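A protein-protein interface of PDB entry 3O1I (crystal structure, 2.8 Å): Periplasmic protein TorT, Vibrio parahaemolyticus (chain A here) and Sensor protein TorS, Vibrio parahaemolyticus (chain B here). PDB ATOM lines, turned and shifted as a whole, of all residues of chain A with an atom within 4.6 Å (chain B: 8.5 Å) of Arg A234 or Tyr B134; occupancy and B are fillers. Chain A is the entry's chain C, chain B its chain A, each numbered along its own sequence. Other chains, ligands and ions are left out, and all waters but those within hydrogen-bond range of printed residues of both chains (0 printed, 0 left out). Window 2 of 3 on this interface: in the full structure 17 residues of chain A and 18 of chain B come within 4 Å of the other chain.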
ATOM      1  N   HIS A 230      -0.942  35.457  -9.710  1.00  0.00           N
ATOM      2  CA  HIS A 230      -2.335  35.037  -9.662  1.00  0.00           C
ATOM      3  C   HIS A 230      -2.927  34.803 -11.042  1.00  0.00           C
ATOM      4  O   HIS A 230      -3.942  34.125 -11.184  1.00  0.00           O
ATOM      5  CB  HIS A 230      -3.188  36.071  -8.927  1.00  0.00           C
ATOM      6  CG  HIS A 230      -2.776  36.299  -7.507  1.00  0.00           C
ATOM      7  ND1 HIS A 230      -3.658  36.193  -6.450  1.00  0.00           N
ATOM      8  CD2 HIS A 230      -1.584  36.647  -6.968  1.00  0.00           C
ATOM      9  CE1 HIS A 230      -3.026  36.466  -5.322  1.00  0.00           C
ATOM     10  NE2 HIS A 230      -1.767  36.747  -5.607  1.00  0.00           N
ATOM     11  N   GLY A 231      -2.298  35.367 -12.064  1.00  0.00           N
ATOM     12  CA  GLY A 231      -2.816  35.198 -13.408  1.00  0.00           C
ATOM     13  C   GLY A 231      -2.259  33.951 -14.040  1.00  0.00           C
ATOM     14  O   GLY A 231      -3.000  33.157 -14.624  1.00  0.00           O
ATOM     15  N   VAL A 232      -0.943  33.788 -13.928  1.00  0.00           N
ATOM     16  CA  VAL A 232      -0.264  32.613 -14.469  1.00  0.00           C
ATOM     17  C   VAL A 232      -0.780  31.359 -13.755  1.00  0.00           C
ATOM     18  O   VAL A 232      -0.793  30.277 -14.327  1.00  0.00           O
ATOM     19  CB  VAL A 232       1.267  32.725 -14.311  1.00  0.00           C
ATOM     20  CG1 VAL A 232       1.942  31.432 -14.735  1.00  0.00           C
ATOM     21  CG2 VAL A 232       1.779  33.881 -15.161  1.00  0.00           C
ATOM     22  N   TYR A 233      -1.215  31.518 -12.507  1.00  0.00           N
ATOM     23  CA  TYR A 233      -1.765  30.406 -11.742  1.00  0.00           C
ATOM     24  C   TYR A 233      -3.096  29.994 -12.360  1.00  0.00           C
ATOM     25  O   TYR A 233      -3.255  28.842 -12.756  1.00  0.00           O
ATOM     26  CB  TYR A 233      -1.982  30.791 -10.278  1.00  0.00           C
ATOM     27  CG  TYR A 233      -2.767  29.760  -9.495  1.00  0.00           C
ATOM     28  CD1 TYR A 233      -2.195  28.532  -9.121  1.00  0.00           C
ATOM     29  CD2 TYR A 233      -4.099  29.999  -9.146  1.00  0.00           C
ATOM     30  CE1 TYR A 233      -2.937  27.571  -8.415  1.00  0.00           C
ATOM     31  CE2 TYR A 233      -4.844  29.056  -8.448  1.00  0.00           C
ATOM     32  CZ  TYR A 233      -4.265  27.848  -8.084  1.00  0.00           C
ATOM     33  OH  TYR A 233      -5.036  26.946  -7.385  1.00  0.00           O
ATOM     34  N   ARG A 234      -4.047  30.925 -12.452  1.00  0.00           N
ATOM     35  CA  ARG A 234      -5.356  30.616 -13.037  1.00  0.00           C
ATOM     36  C   ARG A 234      -5.192  29.946 -14.406  1.00  0.00           C
ATOM     37  O   ARG A 234      -6.038  29.154 -14.840  1.00  0.00           O
ATOM     38  CB  ARG A 234      -6.196  31.878 -13.216  1.00  0.00           C
ATOM     39  CG  ARG A 234      -7.666  31.571 -13.328  1.00  0.00           C
ATOM     40  CD  ARG A 234      -8.421  32.660 -14.036  1.00  0.00           C
ATOM     41  NE  ARG A 234      -8.648  32.384 -15.460  1.00  0.00           N
ATOM     42  CZ  ARG A 234      -7.723  32.454 -16.418  1.00  0.00           C
ATOM     43  NH1 ARG A 234      -6.463  32.791 -16.143  1.00  0.00           N
ATOM     44  NH2 ARG A 234      -8.071  32.211 -17.671  1.00  0.00           N
ATOM     45  N   GLY A 235      -4.098  30.279 -15.083  1.00  0.00           N
ATOM     46  CA  GLY A 235      -3.834  29.701 -16.388  1.00  0.00           C
ATOM     47  C   GLY A 235      -3.425  28.249 -16.265  1.00  0.00           C
ATOM     48  O   GLY A 235      -3.786  27.416 -17.101  1.00  0.00           O
ATOM     49  N   LEU A 236      -2.648  27.950 -15.230  1.00  0.00           N
ATOM     50  CA  LEU A 236      -2.213  26.588 -14.980  1.00  0.00           C
ATOM     51  C   LEU A 236      -3.464  25.784 -14.656  1.00  0.00           C
ATOM     52  O   LEU A 236      -3.656  24.688 -15.171  1.00  0.00           O
ATOM     53  CB  LEU A 236      -1.239  26.555 -13.805  1.00  0.00           C
ATOM     54  CG  LEU A 236       0.144  27.081 -14.175  1.00  0.00           C
ATOM     55  CD1 LEU A 236       0.952  27.309 -12.927  1.00  0.00           C
ATOM     56  CD2 LEU A 236       0.839  26.102 -15.107  1.00  0.00           C
ATOM     57  N   LEU A 237      -4.323  26.353 -13.816  1.00  0.00           N
ATOM     58  CA  LEU A 237      -5.566  25.708 -13.419  1.00  0.00           C
ATOM     59  C   LEU A 237      -6.489  25.386 -14.603  1.00  0.00           C
ATOM     60  O   LEU A 237      -7.424  24.596 -14.471  1.00  0.00           O
ATOM     61  CB  LEU A 237      -6.318  26.611 -12.442  1.00  0.00           C
ATOM     62  CG  LEU A 237      -7.510  25.948 -11.758  1.00  0.00           C
ATOM     63  CD1 LEU A 237      -6.978  25.081 -10.635  1.00  0.00           C
ATOM     64  CD2 LEU A 237      -8.478  26.983 -11.208  1.00  0.00           C
ATOM     65  N   ARG A 238      -6.232  26.001 -15.752  1.00  0.00           N
ATOM     66  CA  ARG A 238      -7.063  25.793 -16.933  1.00  0.00           C
ATOM     67  C   ARG A 238      -6.268  25.416 -18.167  1.00  0.00           C
ATOM     68  O   ARG A 238      -6.672  25.734 -19.284  1.00  0.00           O
ATOM     69  CB  ARG A 238      -7.855  27.058 -17.244  1.00  0.00           C
ATOM     70  CG  ARG A 238      -8.843  27.430 -16.196  1.00  0.00           C
ATOM     71  CD  ARG A 238     -10.024  26.522 -16.260  1.00  0.00           C
ATOM     72  NE  ARG A 238     -10.728  26.610 -14.998  1.00  0.00           N
ATOM     73  CZ  ARG A 238     -11.644  25.747 -14.589  1.00  0.00           C
ATOM     74  NH1 ARG A 238     -11.983  24.718 -15.357  1.00  0.00           N
ATOM     75  NH2 ARG A 238     -12.182  25.896 -13.384  1.00  0.00           N
ATOM     76  N   ALA B 126      -9.248  40.649  -8.817  1.00  0.00           N
ATOM     77  CA  ALA B 126     -10.404  40.279  -9.619  1.00  0.00           C
ATOM     78  C   ALA B 126     -10.117  38.893 -10.174  1.00  0.00           C
ATOM     79  O   ALA B 126     -10.973  38.013 -10.145  1.00  0.00           O
ATOM     80  CB  ALA B 126     -10.600  41.273 -10.741  1.00  0.00           C
ATOM     81  N   VAL B 127      -8.903  38.709 -10.677  1.00  0.00           N
ATOM     82  CA  VAL B 127      -8.487  37.423 -11.204  1.00  0.00           C
ATOM     83  C   VAL B 127      -8.685  36.384 -10.100  1.00  0.00           C
ATOM     84  O   VAL B 127      -9.333  35.361 -10.302  1.00  0.00           O
ATOM     85  CB  VAL B 127      -7.006  37.460 -11.612  1.00  0.00           C
ATOM     86  CG1 VAL B 127      -6.523  36.072 -11.986  1.00  0.00           C
ATOM     87  CG2 VAL B 127      -6.822  38.413 -12.768  1.00  0.00           C
ATOM     88  N   ALA B 128      -8.136  36.672  -8.927  1.00  0.00           N
ATOM     89  CA  ALA B 128      -8.246  35.785  -7.777  1.00  0.00           C
ATOM     90  C   ALA B 128      -9.700  35.516  -7.407  1.00  0.00           C
ATOM     91  O   ALA B 128     -10.141  34.375  -7.393  1.00  0.00           O
ATOM     92  CB  ALA B 128      -7.506  36.392  -6.590  1.00  0.00           C
ATOM     93  N   ASN B 129     -10.444  36.568  -7.104  1.00  0.00           N
ATOM     94  CA  ASN B 129     -11.848  36.420  -6.744  1.00  0.00           C
ATOM     95  C   ASN B 129     -12.607  35.526  -7.728  1.00  0.00           C
ATOM     96  O   ASN B 129     -13.643  34.951  -7.384  1.00  0.00           O
ATOM     97  CB  ASN B 129     -12.517  37.799  -6.666  1.00  0.00           C
ATOM     98  CG  ASN B 129     -12.205  38.528  -5.367  1.00  0.00           C
ATOM     99  OD1 ASN B 129     -11.089  38.445  -4.840  1.00  0.00           O
ATOM    100  ND2 ASN B 129     -13.192  39.255  -4.850  1.00  0.00           N
ATOM    101  N   VAL B 130     -12.092  35.418  -8.952  1.00  0.00           N
ATOM    102  CA  VAL B 130     -12.712  34.594  -9.983  1.00  0.00           C
ATOM    103  C   VAL B 130     -12.125  33.193  -9.919  1.00  0.00           C
ATOM    104  O   VAL B 130     -12.857  32.202  -9.964  1.00  0.00           O
ATOM    105  CB  VAL B 130     -12.505  35.208 -11.399  1.00  0.00           C
ATOM    106  CG1 VAL B 130     -12.304  34.109 -12.441  1.00  0.00           C
ATOM    107  CG2 VAL B 130     -13.726  36.036 -11.772  1.00  0.00           C
ATOM    108  N   THR B 131     -10.804  33.114  -9.808  1.00  0.00           N
ATOM    109  CA  THR B 131     -10.141  31.826  -9.720  1.00  0.00           C
ATOM    110  C   THR B 131     -10.758  31.046  -8.570  1.00  0.00           C
ATOM    111  O   THR B 131     -10.710  29.817  -8.530  1.00  0.00           O
ATOM    112  CB  THR B 131      -8.662  31.983  -9.425  1.00  0.00           C
ATOM    113  OG1 THR B 131      -8.073  32.835 -10.406  1.00  0.00           O
ATOM    114  CG2 THR B 131      -7.983  30.632  -9.465  1.00  0.00           C
ATOM    115  N   HIS B 132     -11.332  31.782  -7.629  1.00  0.00           N
ATOM    116  CA  HIS B 132     -11.958  31.196  -6.463  1.00  0.00           C
ATOM    117  C   HIS B 132     -13.367  30.726  -6.798  1.00  0.00           C
ATOM    118  O   HIS B 132     -13.913  29.850  -6.133  1.00  0.00           O
ATOM    119  CB  HIS B 132     -12.020  32.231  -5.356  1.00  0.00           C
ATOM    120  CG  HIS B 132     -12.591  31.712  -4.077  1.00  0.00           C
ATOM    121  ND1 HIS B 132     -11.864  30.938  -3.199  1.00  0.00           N
ATOM    122  CD2 HIS B 132     -13.813  31.879  -3.517  1.00  0.00           C
ATOM    123  CE1 HIS B 132     -12.612  30.656  -2.148  1.00  0.00           C
ATOM    124  NE2 HIS B 132     -13.799  31.215  -2.316  1.00  0.00           N
ATOM    125  N   ILE B 133     -13.965  31.328  -7.817  1.00  0.00           N
ATOM    126  CA  ILE B 133     -15.298  30.933  -8.233  1.00  0.00           C
ATOM    127  C   ILE B 133     -15.153  29.509  -8.759  1.00  0.00           C
ATOM    128  O   ILE B 133     -16.035  28.673  -8.573  1.00  0.00           O
ATOM    129  CB  ILE B 133     -15.822  31.817  -9.379  1.00  0.00           C
ATOM    130  CG1 ILE B 133     -15.631  33.297  -9.045  1.00  0.00           C
ATOM    131  CG2 ILE B 133     -17.299  31.521  -9.616  1.00  0.00           C
ATOM    132  CD1 ILE B 133     -16.631  33.856  -8.056  1.00  0.00           C
ATOM    133  N   TYR B 134     -14.022  29.253  -9.419  1.00  0.00           N
ATOM    134  CA  TYR B 134     -13.711  27.942  -9.994  1.00  0.00           C
ATOM    135  C   TYR B 134     -13.812  26.838  -8.946  1.00  0.00           C
ATOM    136  O   TYR B 134     -14.703  25.990  -9.005  1.00  0.00           O
ATOM    137  CB  TYR B 134     -12.291  27.930 -10.587  1.00  0.00           C
ATOM    138  CG  TYR B 134     -12.104  28.693 -11.889  1.00  0.00           C
ATOM    139  CD1 TYR B 134     -10.823  28.992 -12.361  1.00  0.00           C
ATOM    140  CD2 TYR B 134     -13.200  29.099 -12.657  1.00  0.00           C
ATOM    141  CE1 TYR B 134     -10.635  29.676 -13.564  1.00  0.00           C
ATOM    142  CE2 TYR B 134     -13.022  29.785 -13.862  1.00  0.00           C
ATOM    143  CZ  TYR B 134     -11.737  30.071 -14.307  1.00  0.00           C
ATOM    144  OH  TYR B 134     -11.556  30.761 -15.488  1.00  0.00           O
ATOM    145  N   ASP B 135     -12.886  26.854  -7.991  1.00  0.00           N
ATOM    146  CA  ASP B 135     -12.855  25.854  -6.932  1.00  0.00           C
ATOM    147  C   ASP B 135     -14.205  25.772  -6.226  1.00  0.00           C
ATOM    148  O   ASP B 135     -14.665  24.689  -5.861  1.00  0.00           O
ATOM    149  CB  ASP B 135     -11.753  26.190  -5.920  1.00  0.00           C
ATOM    150  CG  ASP B 135     -10.401  26.429  -6.584  1.00  0.00           C
ATOM    151  OD1 ASP B 135     -10.180  25.907  -7.702  1.00  0.00           O
ATOM    152  OD2 ASP B 135      -9.554  27.129  -5.983  1.00  0.00           O
ATOM    153  N   LEU B 136     -14.835  26.926  -6.042  1.00  0.00           N
ATOM    154  CA  LEU B 136     -16.138  27.006  -5.391  1.00  0.00           C
ATOM    155  C   LEU B 136     -17.215  26.323  -6.241  1.00  0.00           C
ATOM    156  O   LEU B 136     -18.189  25.793  -5.715  1.00  0.00           O
ATOM    157  CB  LEU B 136     -16.507  28.477  -5.157  1.00  0.00           C
ATOM    158  CG  LEU B 136     -17.895  28.803  -4.607  1.00  0.00           C
ATOM    159  CD1 LEU B 136     -18.036  28.248  -3.210  1.00  0.00           C
ATOM    160  CD2 LEU B 136     -18.100  30.300  -4.600  1.00  0.00           C
ATOM    161  N   LEU B 137     -17.030  26.333  -7.556  1.00  0.00           N
ATOM    162  CA  LEU B 137     -17.991  25.725  -8.469  1.00  0.00           C
ATOM    163  C   LEU B 137     -17.901  24.208  -8.475  1.00  0.00           C
ATOM    164  O   LEU B 137     -18.912  23.513  -8.377  1.00  0.00           O
ATOM    165  CB  LEU B 137     -17.764  26.248  -9.888  1.00  0.00           C
ATOM    166  CG  LEU B 137     -18.669  25.698 -10.989  1.00  0.00           C
ATOM    167  CD1 LEU B 137     -20.125  26.011 -10.680  1.00  0.00           C
ATOM    168  CD2 LEU B 137     -18.269  26.316 -12.305  1.00  0.00           C
ATOM    169  N   GLU B 138     -16.682  23.700  -8.605  1.00  0.00           N
ATOM    170  CA  GLU B 138     -16.443  22.265  -8.639  1.00  0.00           C
ATOM    171  C   GLU B 138     -17.072  21.561  -7.436  1.00  0.00           C
ATOM    172  O   GLU B 138     -17.721  20.525  -7.588  1.00  0.00           O
ATOM    173  CB  GLU B 138     -14.941  22.004  -8.682  1.00  0.00           C
ATOM    174  CG  GLU B 138     -14.576  20.568  -8.938  1.00  0.00           C
ATOM    175  CD  GLU B 138     -13.080  20.370  -9.048  1.00  0.00           C
ATOM    176  OE1 GLU B 138     -12.335  20.629  -8.101  1.00  0.00           O
ATOM    177  OE2 GLU B 138     -12.630  19.911 -10.210  1.00  0.00           O
ATOM    178  N   ALA B 139     -16.882  22.127  -6.247  1.00  0.00           N
ATOM    179  CA  ALA B 139     -17.441  21.562  -5.022  1.00  0.00           C
ATOM    180  C   ALA B 139     -18.974  21.623  -5.057  1.00  0.00           C
ATOM    181  O   ALA B 139     -19.646  21.181  -4.125  1.00  0.00           O
ATOM    182  CB  ALA B 139     -16.909  22.318  -3.806  1.00  0.00           C
ATOM    183  N   ASN B 140     -19.512  22.189  -6.134  1.00  0.00           N
ATOM    184  CA  ASN B 140     -20.955  22.306  -6.338  1.00  0.00           C
ATOM    185  C   ASN B 140     -21.733  23.184  -5.358  1.00  0.00           C
ATOM    186  O   ASN B 140     -22.962  23.095  -5.298  1.00  0.00           O
ATOM    187  CB  ASN B 140     -21.592  20.915  -6.363  1.00  0.00           C
ATOM    188  CG  ASN B 140     -21.023  20.033  -7.450  1.00  0.00           C
ATOM    189  OD1 ASN B 140     -20.955  20.431  -8.613  1.00  0.00           O
ATOM    190  ND2 ASN B 140     -20.615  18.826  -7.082  1.00  0.00           N
ATOM    191  N   LYS B 141     -21.046  24.031  -4.595  1.00  0.00           N
ATOM    192  CA  LYS B 141     -21.744  24.900  -3.649  1.00  0.00           C
ATOM    193  C   LYS B 141     -22.345  26.072  -4.423  1.00  0.00           C
ATOM    194  O   LYS B 141     -22.159  27.236  -4.087  1.00  0.00           O
ATOM    195  CB  LYS B 141     -20.777  25.375  -2.556  1.00  0.00           C
ATOM    196  CG  LYS B 141     -20.100  24.212  -1.842  1.00  0.00           C
ATOM    197  CD  LYS B 141     -19.420  24.592  -0.541  1.00  0.00           C
ATOM    198  CE  LYS B 141     -18.922  23.328   0.168  1.00  0.00           C
ATOM    199  NZ  LYS B 141     -18.340  23.580   1.518  1.00  0.00           N
ATOM    200  N   VAL B 145     -21.408  30.121  -5.112  1.00  0.00           N
ATOM    201  CA  VAL B 145     -20.904  30.575  -6.405  1.00  0.00           C
ATOM    202  C   VAL B 145     -21.778  31.720  -6.898  1.00  0.00           C
ATOM    203  O   VAL B 145     -21.306  32.627  -7.585  1.00  0.00           O
ATOM    204  CB  VAL B 145     -20.927  29.454  -7.459  1.00  0.00           C
ATOM    205  CG1 VAL B 145     -20.488  30.001  -8.807  1.00  0.00           C
ATOM    206  CG2 VAL B 145     -20.009  28.326  -7.038  1.00  0.00           C
ATOM    207  N   ALA B 148     -20.658  34.746  -4.782  1.00  0.00           N
ATOM    208  CA  ALA B 148     -19.331  35.102  -5.268  1.00  0.00           C
ATOM    209  C   ALA B 148     -19.370  35.813  -6.612  1.00  0.00           C
ATOM    210  O   ALA B 148     -18.406  36.484  -6.985  1.00  0.00           O
ATOM    211  CB  ALA B 148     -18.459  33.869  -5.362  1.00  0.00           C
ATOM    212  N   LEU B 149     -20.471  35.654  -7.341  1.00  0.00           N
ATOM    213  CA  LEU B 149     -20.625  36.316  -8.630  1.00  0.00           C
ATOM    214  C   LEU B 149     -21.178  37.712  -8.409  1.00  0.00           C
ATOM    215  O   LEU B 149     -20.741  38.662  -9.041  1.00  0.00           O
ATOM    216  CB  LEU B 149     -21.575  35.542  -9.543  1.00  0.00           C
ATOM    217  CG  LEU B 149     -21.057  34.263 -10.199  1.00  0.00           C
ATOM    218  CD1 LEU B 149     -22.124  33.732 -11.136  1.00  0.00           C
ATOM    219  CD2 LEU B 149     -19.779  34.545 -10.971  1.00  0.00           C
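The side-chain hydroxyl (OH) of Tyr B134 is in hydrogen-bond range of the guanidinium group (NE) of Arg A234, 3.3 Å away.
The side-chain hydroxyl (OG1) of Thr B131 lies within hydrogen-bond range of the backbone carbonyl oxygen (O) of Val B127, at 2.8 Å.
Among the printed residues, merely in contact across the chains: Arg A238 with Tyr B134 (3.2 Å), Arg A234 with Thr B131 (3.2 Å), Leu A237 with Tyr B134 (3.3 Å), His A230 with Val B127 (3.3 Å), Tyr A233 with Thr B131 (3.7 Å) and His A230 with Ala B128 (3.9 Å).
Printed residues of chain B within 4 Å of His A230: Val B127 and Ala B128.
No residue of chain B comes within 4 Å of Gly A235.
Printed residues of chain B within 4 Å of Leu A237: Tyr B134.
Printed residues of chain A within 4 Å of Val B127: His A230 (3.3 Å).
Printed residues of chain A within 4 Å of Ala B128: His A230 (3.9 Å).
Tyr B134 touches just these residues of chain A: Arg A234 (3.3 Å), Leu A237 (3.3 Å) and Arg A238 (3.2 Å).
The nearest residue of chain B that does not touch Arg A234 is Val B127 (4.4 Å).
The nearest printed residue of chain A that does not touch Thr B131 is Leu A237 (4.1 Å).
Of the 9 printed residues of chain A, 5 touch a printed residue of chain B.
Of the 19 printed residues of chain B, 4 touch a printed residue of chain A.
Hydrophobic or aromatic side chains of chain B that line the printed part of chain A: Val B127, Ala B128 and Tyr B134.
Among the printed residues, 7 pairs touch across the chains.
Among the printed residues, no Asp or Glu carboxylate lies within 4 Å of a Lys or Arg side-chain nitrogen of the other chain.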
